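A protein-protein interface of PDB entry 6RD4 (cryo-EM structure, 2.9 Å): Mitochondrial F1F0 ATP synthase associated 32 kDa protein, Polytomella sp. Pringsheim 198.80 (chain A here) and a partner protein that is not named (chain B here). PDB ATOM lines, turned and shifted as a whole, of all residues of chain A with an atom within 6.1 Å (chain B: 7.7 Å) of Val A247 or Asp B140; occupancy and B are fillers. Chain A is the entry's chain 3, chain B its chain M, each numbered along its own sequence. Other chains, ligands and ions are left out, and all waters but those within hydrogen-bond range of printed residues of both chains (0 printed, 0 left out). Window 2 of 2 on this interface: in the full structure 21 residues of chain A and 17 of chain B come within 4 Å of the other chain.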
ATOM      1  N   VAL A 212       3.479   8.121 -18.426  1.00  0.00           N
ATOM      2  CA  VAL A 212       3.356   7.385 -17.178  1.00  0.00           C
ATOM      3  C   VAL A 212       4.575   7.608 -16.293  1.00  0.00           C
ATOM      4  O   VAL A 212       4.484   7.559 -15.064  1.00  0.00           O
ATOM      5  CB  VAL A 212       3.121   5.913 -17.530  1.00  0.00           C
ATOM      6  CG1 VAL A 212       2.924   5.100 -16.342  1.00  0.00           C
ATOM      7  CG2 VAL A 212       1.907   5.801 -18.376  1.00  0.00           C
ATOM      8  N   ARG A 213       5.714   7.909 -16.888  1.00  0.00           N
ATOM      9  CA  ARG A 213       6.937   8.212 -16.171  1.00  0.00           C
ATOM     10  C   ARG A 213       7.097   9.680 -15.851  1.00  0.00           C
ATOM     11  O   ARG A 213       8.201  10.099 -15.512  1.00  0.00           O
ATOM     12  CB  ARG A 213       8.138   7.767 -16.993  1.00  0.00           C
ATOM     13  CG  ARG A 213       8.430   6.308 -16.911  1.00  0.00           C
ATOM     14  CD  ARG A 213       9.323   6.022 -15.744  1.00  0.00           C
ATOM     15  NE  ARG A 213       9.779   4.655 -15.789  1.00  0.00           N
ATOM     16  CZ  ARG A 213       9.104   3.643 -15.281  1.00  0.00           C
ATOM     17  NH1 ARG A 213       9.576   2.419 -15.379  1.00  0.00           N
ATOM     18  NH2 ARG A 213       7.960   3.860 -14.660  1.00  0.00           N
ATOM     19  N   SER A 245      -3.093   8.703 -12.900  1.00  0.00           N
ATOM     20  CA  SER A 245      -3.607   7.512 -12.265  1.00  0.00           C
ATOM     21  C   SER A 245      -3.489   7.695 -10.765  1.00  0.00           C
ATOM     22  O   SER A 245      -3.086   8.754 -10.285  1.00  0.00           O
ATOM     23  CB  SER A 245      -2.862   6.267 -12.746  1.00  0.00           C
ATOM     24  OG  SER A 245      -3.379   5.107 -12.127  1.00  0.00           O
ATOM     25  N   GLU A 246      -3.853   6.657 -10.022  1.00  0.00           N
ATOM     26  CA  GLU A 246      -3.615   6.656  -8.590  1.00  0.00           C
ATOM     27  C   GLU A 246      -2.135   6.635  -8.280  1.00  0.00           C
ATOM     28  O   GLU A 246      -1.708   7.168  -7.253  1.00  0.00           O
ATOM     29  CB  GLU A 246      -4.285   5.448  -7.959  1.00  0.00           C
ATOM     30  CG  GLU A 246      -5.776   5.546  -7.888  1.00  0.00           C
ATOM     31  CD  GLU A 246      -6.454   5.084  -9.150  1.00  0.00           C
ATOM     32  OE1 GLU A 246      -5.750   4.667 -10.086  1.00  0.00           O
ATOM     33  OE2 GLU A 246      -7.697   5.145  -9.211  1.00  0.00           O
ATOM     34  N   VAL A 247      -1.346   6.032  -9.167  1.00  0.00           N
ATOM     35  CA  VAL A 247       0.091   5.944  -8.982  1.00  0.00           C
ATOM     36  C   VAL A 247       0.733   7.305  -9.126  1.00  0.00           C
ATOM     37  O   VAL A 247       1.553   7.711  -8.301  1.00  0.00           O
ATOM     38  CB  VAL A 247       0.678   4.958  -9.994  1.00  0.00           C
ATOM     39  CG1 VAL A 247       2.118   4.726  -9.691  1.00  0.00           C
ATOM     40  CG2 VAL A 247      -0.111   3.686 -10.014  1.00  0.00           C
ATOM     41  N   SER A 248       0.389   8.025 -10.182  1.00  0.00           N
ATOM     42  CA  SER A 248       1.083   9.261 -10.494  1.00  0.00           C
ATOM     43  C   SER A 248       0.667  10.396  -9.583  1.00  0.00           C
ATOM     44  O   SER A 248       1.493  11.254  -9.265  1.00  0.00           O
ATOM     45  CB  SER A 248       0.838   9.627 -11.946  1.00  0.00           C
ATOM     46  OG  SER A 248      -0.538   9.553 -12.239  1.00  0.00           O
ATOM     47  N   LEU A 249      -0.591  10.415  -9.157  1.00  0.00           N
ATOM     48  CA  LEU A 249      -1.077  11.408  -8.216  1.00  0.00           C
ATOM     49  C   LEU A 249      -0.757  11.055  -6.777  1.00  0.00           C
ATOM     50  O   LEU A 249      -0.625  11.959  -5.951  1.00  0.00           O
ATOM     51  CB  LEU A 249      -2.584  11.588  -8.374  1.00  0.00           C
ATOM     52  CG  LEU A 249      -3.037  12.220  -9.679  1.00  0.00           C
ATOM     53  CD1 LEU A 249      -4.431  11.798  -9.986  1.00  0.00           C
ATOM     54  CD2 LEU A 249      -2.959  13.718  -9.601  1.00  0.00           C
ATOM     55  N   GLY A 250      -0.593   9.772  -6.461  1.00  0.00           N
ATOM     56  CA  GLY A 250      -0.188   9.376  -5.127  1.00  0.00           C
ATOM     57  C   GLY A 250       1.227   9.768  -4.764  1.00  0.00           C
ATOM     58  O   GLY A 250       1.556   9.832  -3.579  1.00  0.00           O
ATOM     59  N   LYS A 251       2.070  10.043  -5.748  1.00  0.00           N
ATOM     60  CA  LYS A 251       3.420  10.508  -5.483  1.00  0.00           C
ATOM     61  C   LYS A 251       3.481  12.002  -5.233  1.00  0.00           C
ATOM     62  O   LYS A 251       4.575  12.537  -5.037  1.00  0.00           O
ATOM     63  CB  LYS A 251       4.339  10.146  -6.646  1.00  0.00           C
ATOM     64  CG  LYS A 251       4.391   8.666  -6.897  1.00  0.00           C
ATOM     65  CD  LYS A 251       5.180   8.330  -8.128  1.00  0.00           C
ATOM     66  CE  LYS A 251       5.066   6.853  -8.426  1.00  0.00           C
ATOM     67  NZ  LYS A 251       5.932   6.451  -9.548  1.00  0.00           N
ATOM     68  N   LEU A 252       2.344  12.678  -5.239  1.00  0.00           N
ATOM     69  CA  LEU A 252       2.259  14.103  -4.990  1.00  0.00           C
ATOM     70  C   LEU A 252       1.841  14.351  -3.547  1.00  0.00           C
ATOM     71  O   LEU A 252       1.096  13.571  -2.955  1.00  0.00           O
ATOM     72  CB  LEU A 252       1.246  14.745  -5.933  1.00  0.00           C
ATOM     73  CG  LEU A 252       1.542  14.836  -7.420  1.00  0.00           C
ATOM     74  CD1 LEU A 252       0.285  15.123  -8.179  1.00  0.00           C
ATOM     75  CD2 LEU A 252       2.528  15.932  -7.658  1.00  0.00           C
ATOM     76  N   ARG B 133      -6.521   2.789 -18.728  1.00  0.00           N
ATOM     77  CA  ARG B 133      -6.772   3.027 -17.320  1.00  0.00           C
ATOM     78  C   ARG B 133      -5.787   2.252 -16.464  1.00  0.00           C
ATOM     79  O   ARG B 133      -5.221   2.793 -15.514  1.00  0.00           O
ATOM     80  CB  ARG B 133      -8.204   2.626 -16.988  1.00  0.00           C
ATOM     81  CG  ARG B 133      -8.597   2.823 -15.553  1.00  0.00           C
ATOM     82  CD  ARG B 133      -8.945   4.250 -15.256  1.00  0.00           C
ATOM     83  NE  ARG B 133      -9.160   4.421 -13.832  1.00  0.00           N
ATOM     84  CZ  ARG B 133      -8.225   4.842 -13.000  1.00  0.00           C
ATOM     85  NH1 ARG B 133      -7.034   5.147 -13.467  1.00  0.00           N
ATOM     86  NH2 ARG B 133      -8.477   4.968 -11.714  1.00  0.00           N
ATOM     87  N   LEU B 134      -5.545   1.002 -16.816  1.00  0.00           N
ATOM     88  CA  LEU B 134      -4.729   0.113 -16.016  1.00  0.00           C
ATOM     89  C   LEU B 134      -3.261   0.155 -16.397  1.00  0.00           C
ATOM     90  O   LEU B 134      -2.451  -0.517 -15.766  1.00  0.00           O
ATOM     91  CB  LEU B 134      -5.259  -1.304 -16.158  1.00  0.00           C
ATOM     92  CG  LEU B 134      -5.068  -2.230 -14.978  1.00  0.00           C
ATOM     93  CD1 LEU B 134      -5.884  -1.715 -13.862  1.00  0.00           C
ATOM     94  CD2 LEU B 134      -5.477  -3.614 -15.331  1.00  0.00           C
ATOM     95  N   LEU B 135      -2.893   0.930 -17.407  1.00  0.00           N
ATOM     96  CA  LEU B 135      -1.511   0.925 -17.867  1.00  0.00           C
ATOM     97  C   LEU B 135      -0.518   1.549 -16.900  1.00  0.00           C
ATOM     98  O   LEU B 135       0.609   1.040 -16.839  1.00  0.00           O
ATOM     99  CB  LEU B 135      -1.394   1.595 -19.235  1.00  0.00           C
ATOM    100  CG  LEU B 135      -1.447   0.717 -20.467  1.00  0.00           C
ATOM    101  CD1 LEU B 135      -1.114   1.578 -21.632  1.00  0.00           C
ATOM    102  CD2 LEU B 135      -0.508  -0.443 -20.350  1.00  0.00           C
ATOM    103  N   PRO B 136      -0.808   2.621 -16.154  1.00  0.00           N
ATOM    104  CA  PRO B 136       0.146   3.006 -15.111  1.00  0.00           C
ATOM    105  C   PRO B 136       0.203   2.057 -13.952  1.00  0.00           C
ATOM    106  O   PRO B 136       1.210   2.047 -13.250  1.00  0.00           O
ATOM    107  CB  PRO B 136      -0.354   4.373 -14.667  1.00  0.00           C
ATOM    108  CG  PRO B 136      -1.007   4.866 -15.773  1.00  0.00           C
ATOM    109  CD  PRO B 136      -1.707   3.756 -16.406  1.00  0.00           C
ATOM    110  N   ALA B 137      -0.841   1.284 -13.703  1.00  0.00           N
ATOM    111  CA  ALA B 137      -0.767   0.304 -12.640  1.00  0.00           C
ATOM    112  C   ALA B 137       0.057  -0.891 -13.054  1.00  0.00           C
ATOM    113  O   ALA B 137       0.666  -1.534 -12.203  1.00  0.00           O
ATOM    114  CB  ALA B 137      -2.163  -0.139 -12.241  1.00  0.00           C
ATOM    115  N   VAL B 138       0.092  -1.193 -14.347  1.00  0.00           N
ATOM    116  CA  VAL B 138       0.913  -2.275 -14.872  1.00  0.00           C
ATOM    117  C   VAL B 138       2.370  -1.848 -14.981  1.00  0.00           C
ATOM    118  O   VAL B 138       3.279  -2.629 -14.703  1.00  0.00           O
ATOM    119  CB  VAL B 138       0.321  -2.720 -16.213  1.00  0.00           C
ATOM    120  CG1 VAL B 138       1.242  -3.597 -16.959  1.00  0.00           C
ATOM    121  CG2 VAL B 138      -0.948  -3.449 -15.964  1.00  0.00           C
ATOM    122  N   VAL B 139       2.620  -0.599 -15.361  1.00  0.00           N
ATOM    123  CA  VAL B 139       3.979  -0.081 -15.411  1.00  0.00           C
ATOM    124  C   VAL B 139       4.550   0.064 -14.009  1.00  0.00           C
ATOM    125  O   VAL B 139       5.725  -0.222 -13.775  1.00  0.00           O
ATOM    126  CB  VAL B 139       3.984   1.242 -16.192  1.00  0.00           C
ATOM    127  CG1 VAL B 139       5.237   2.024 -15.988  1.00  0.00           C
ATOM    128  CG2 VAL B 139       3.818   0.956 -17.625  1.00  0.00           C
ATOM    129  N   ASP B 140       3.724   0.464 -13.043  1.00  0.00           N
ATOM    130  CA  ASP B 140       4.188   0.531 -11.660  1.00  0.00           C
ATOM    131  C   ASP B 140       4.322  -0.844 -11.044  1.00  0.00           C
ATOM    132  O   ASP B 140       5.107  -1.026 -10.116  1.00  0.00           O
ATOM    133  CB  ASP B 140       3.240   1.360 -10.817  1.00  0.00           C
ATOM    134  CG  ASP B 140       3.783   1.655  -9.444  1.00  0.00           C
ATOM    135  OD1 ASP B 140       4.769   2.410  -9.336  1.00  0.00           O
ATOM    136  OD2 ASP B 140       3.207   1.145  -8.464  1.00  0.00           O
ATOM    137  N   ALA B 141       3.564  -1.821 -11.529  1.00  0.00           N
ATOM    138  CA  ALA B 141       3.771  -3.185 -11.077  1.00  0.00           C
ATOM    139  C   ALA B 141       5.094  -3.728 -11.573  1.00  0.00           C
ATOM    140  O   ALA B 141       5.705  -4.564 -10.914  1.00  0.00           O
ATOM    141  CB  ALA B 141       2.636  -4.078 -11.543  1.00  0.00           C
ATOM    142  N   SER B 142       5.548  -3.274 -12.737  1.00  0.00           N
ATOM    143  CA  SER B 142       6.851  -3.677 -13.240  1.00  0.00           C
ATOM    144  C   SER B 142       7.975  -2.889 -12.605  1.00  0.00           C
ATOM    145  O   SER B 142       9.112  -3.353 -12.591  1.00  0.00           O
ATOM    146  CB  SER B 142       6.911  -3.505 -14.741  1.00  0.00           C
ATOM    147  OG  SER B 142       5.950  -4.320 -15.355  1.00  0.00           O
ATOM    148  N   ASP B 143       7.703  -1.691 -12.107  1.00  0.00           N
ATOM    149  CA  ASP B 143       8.745  -0.926 -11.446  1.00  0.00           C
ATOM    150  C   ASP B 143       9.044  -1.434 -10.063  1.00  0.00           C
ATOM    151  O   ASP B 143      10.073  -1.073  -9.495  1.00  0.00           O
ATOM    152  CB  ASP B 143       8.360   0.539 -11.317  1.00  0.00           C
ATOM    153  CG  ASP B 143       8.418   1.270 -12.612  1.00  0.00           C
ATOM    154  OD1 ASP B 143       8.808   0.662 -13.627  1.00  0.00           O
ATOM    155  OD2 ASP B 143       8.101   2.475 -12.610  1.00  0.00           O
ATOM    156  N   LYS B 144       8.153  -2.211  -9.490  1.00  0.00           N
ATOM    157  CA  LYS B 144       8.324  -2.713  -8.149  1.00  0.00           C
ATOM    158  C   LYS B 144       8.762  -4.160  -8.130  1.00  0.00           C
ATOM    159  O   LYS B 144       9.116  -4.669  -7.072  1.00  0.00           O
ATOM    160  CB  LYS B 144       7.031  -2.524  -7.367  1.00  0.00           C
ATOM    161  CG  LYS B 144       6.707  -1.065  -7.133  1.00  0.00           C
ATOM    162  CD  LYS B 144       5.491  -0.882  -6.276  1.00  0.00           C
ATOM    163  CE  LYS B 144       4.296  -1.559  -6.883  1.00  0.00           C
ATOM    164  NZ  LYS B 144       3.064  -1.236  -6.136  1.00  0.00           N
ATOM    165  N   ARG B 145       8.747  -4.829  -9.269  1.00  0.00           N
ATOM    166  CA  ARG B 145       9.280  -6.169  -9.364  1.00  0.00           C
ATOM    167  C   ARG B 145      10.782  -6.108  -9.522  1.00  0.00           C
ATOM    168  O   ARG B 145      11.313  -5.210 -10.171  1.00  0.00           O
ATOM    169  CB  ARG B 145       8.663  -6.904 -10.534  1.00  0.00           C
ATOM    170  CG  ARG B 145       7.287  -7.331 -10.246  1.00  0.00           C
ATOM    171  CD  ARG B 145       6.573  -7.828 -11.443  1.00  0.00           C
ATOM    172  NE  ARG B 145       6.955  -9.192 -11.734  1.00  0.00           N
ATOM    173  CZ  ARG B 145       7.605  -9.549 -12.826  1.00  0.00           C
ATOM    174  NH1 ARG B 145       7.926 -10.812 -13.019  1.00  0.00           N
ATOM    175  NH2 ARG B 145       7.926  -8.635 -13.723  1.00  0.00           N
ATOM    176  N   ASP B 313       4.167  -7.265  -4.554  1.00  0.00           N
ATOM    177  CA  ASP B 313       3.664  -6.003  -4.050  1.00  0.00           C
ATOM    178  C   ASP B 313       2.198  -5.862  -4.400  1.00  0.00           C
ATOM    179  O   ASP B 313       1.625  -6.672  -5.127  1.00  0.00           O
ATOM    180  CB  ASP B 313       4.447  -4.811  -4.589  1.00  0.00           C
ATOM    181  CG  ASP B 313       5.699  -4.554  -3.816  1.00  0.00           C
ATOM    182  OD1 ASP B 313       5.729  -4.912  -2.626  1.00  0.00           O
ATOM    183  OD2 ASP B 313       6.643  -3.963  -4.363  1.00  0.00           O
ATOM    184  N   LYS B 314       1.594  -4.817  -3.852  1.00  0.00           N
ATOM    185  CA  LYS B 314       0.171  -4.584  -4.012  1.00  0.00           C
ATOM    186  C   LYS B 314      -0.093  -3.929  -5.353  1.00  0.00           C
ATOM    187  O   LYS B 314       0.565  -2.949  -5.707  1.00  0.00           O
ATOM    188  CB  LYS B 314      -0.345  -3.693  -2.887  1.00  0.00           C
ATOM    189  CG  LYS B 314      -1.830  -3.816  -2.620  1.00  0.00           C
ATOM    190  CD  LYS B 314      -2.305  -2.715  -1.708  1.00  0.00           C
ATOM    191  CE  LYS B 314      -2.509  -1.423  -2.466  1.00  0.00           C
ATOM    192  NZ  LYS B 314      -3.742  -1.464  -3.297  1.00  0.00           N
ATOM    193  N   PHE B 315      -1.044  -4.470  -6.103  1.00  0.00           N
ATOM    194  CA  PHE B 315      -1.464  -3.816  -7.328  1.00  0.00           C
ATOM    195  C   PHE B 315      -2.248  -2.570  -6.977  1.00  0.00           C
ATOM    196  O   PHE B 315      -3.216  -2.639  -6.222  1.00  0.00           O
ATOM    197  CB  PHE B 315      -2.310  -4.756  -8.169  1.00  0.00           C
ATOM    198  CG  PHE B 315      -2.350  -4.391  -9.608  1.00  0.00           C
ATOM    199  CD1 PHE B 315      -1.299  -4.700 -10.436  1.00  0.00           C
ATOM    200  CD2 PHE B 315      -3.441  -3.751 -10.138  1.00  0.00           C
ATOM    201  CE1 PHE B 315      -1.336  -4.369 -11.754  1.00  0.00           C
ATOM    202  CE2 PHE B 315      -3.476  -3.421 -11.453  1.00  0.00           C
ATOM    203  CZ  PHE B 315      -2.427  -3.733 -12.258  1.00  0.00           C
ATOM    204  N   ILE B 316      -1.820  -1.427  -7.507  1.00  0.00           N
ATOM    205  CA  ILE B 316      -2.423  -0.161  -7.112  1.00  0.00           C
ATOM    206  C   ILE B 316      -3.831  -0.043  -7.673  1.00  0.00           C
ATOM    207  O   ILE B 316      -4.805   0.072  -6.923  1.00  0.00           O
ATOM    208  CB  ILE B 316      -1.541   1.017  -7.540  1.00  0.00           C
ATOM    209  CG1 ILE B 316      -0.234   0.985  -6.768  1.00  0.00           C
ATOM    210  CG2 ILE B 316      -2.232   2.303  -7.258  1.00  0.00           C
ATOM    211  CD1 ILE B 316      -0.405   1.060  -5.287  1.00  0.00           C
ATOM    212  N   GLY B 317      -3.961  -0.078  -8.989  1.00  0.00           N
ATOM    213  CA  GLY B 317      -5.253  -0.248  -9.604  1.00  0.00           C
ATOM    214  C   GLY B 317      -6.154   0.961  -9.510  1.00  0.00           C
ATOM    215  O   GLY B 317      -5.816   1.975  -8.901  1.00  0.00           O
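Pro B136 touches Val A212 (CA to CG1, 3.7 Å).
Val A212 touches Val B139 (CG1 to CG1, 3.9 Å).
Val B139 touches Arg A213.
OG of Ser A245 touches NH1 of Arg B133, 3.9 Å away.
Pro B136 touches Ser A245 (CB to CB, 3.7 Å).
CB of Glu A246 touches CG2 of Ile B316, at 3.8 Å.
CG2 of Val A247 touches O of Pro B136 (3.9 Å).
Val A247 touches Asp B140.
CG2 of Ile B316 touches CG2 of Val A247 (3.7 Å).
OD2 of Asp B143 is in salt-bridge range of NH2 of Arg A213.
OE1 of Glu A246 sits close to O of Gly B317 (2.9 Å).
NH2 of Arg B133 is in salt-bridge range of OE2 of Glu A246, at 2.6 Å.
Val A247 touches three residues of chain B.
Asp B140 touches just one residue of chain A: Val A247 (3.5 Å).
Of the printed residues of chain A, Val B139 touches Val A212 and Arg A213.
Of the printed residues of chain B, Arg A213 touches Val B139 and Asp B143.
Printed residues of chain A within 4 Å of Pro B136: Val A212 (3.7 Å), Ser A245 (3.7 Å) and Val A247 (3.9 Å).
Of the printed residues of chain B, Val A212 touches Pro B136 and Val B139.
Ser B142 touches none of the printed residues of chain A.
The nearest residue of chain B that does not touch Val A247 is Ala B137 (4.3 Å).
The nearest printed residue of chain B that does not touch Ser A245 is Ala B137 (4.9 Å).
OG of Ser A245 is in hydrogen-bond range of OE1 of Glu A246, at 3.2 Å.
N of Ser A245 sits at hydrogen-bond distance from OG of Ser A248 (2.8 Å).
The side-chain amino group of Lys B144 lies within salt-bridge range of the side-chain carboxylate of Asp B140, at 3.3 Å.
Printed residues of chain B that touch a printed residue of chain A: Arg B133, Pro B136, Val B139, Asp B140, Asp B143, Ile B316 and Gly B317.
Hydrophobic or aromatic side chains of chain B that line the printed part of chain A: Pro B136, Val B139 and Ile B316.
Printed residues of chain A that touch a printed residue of chain B: Val A212, Arg A213, Ser A245, Glu A246 and Val A247.
Hydrophobic or aromatic side chains of chain A within 4 Å of the printed part of chain B: Val A212 and Val A247.
Along chain A the printed residues that touch a printed residue of chain B span positions 212 to 247.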
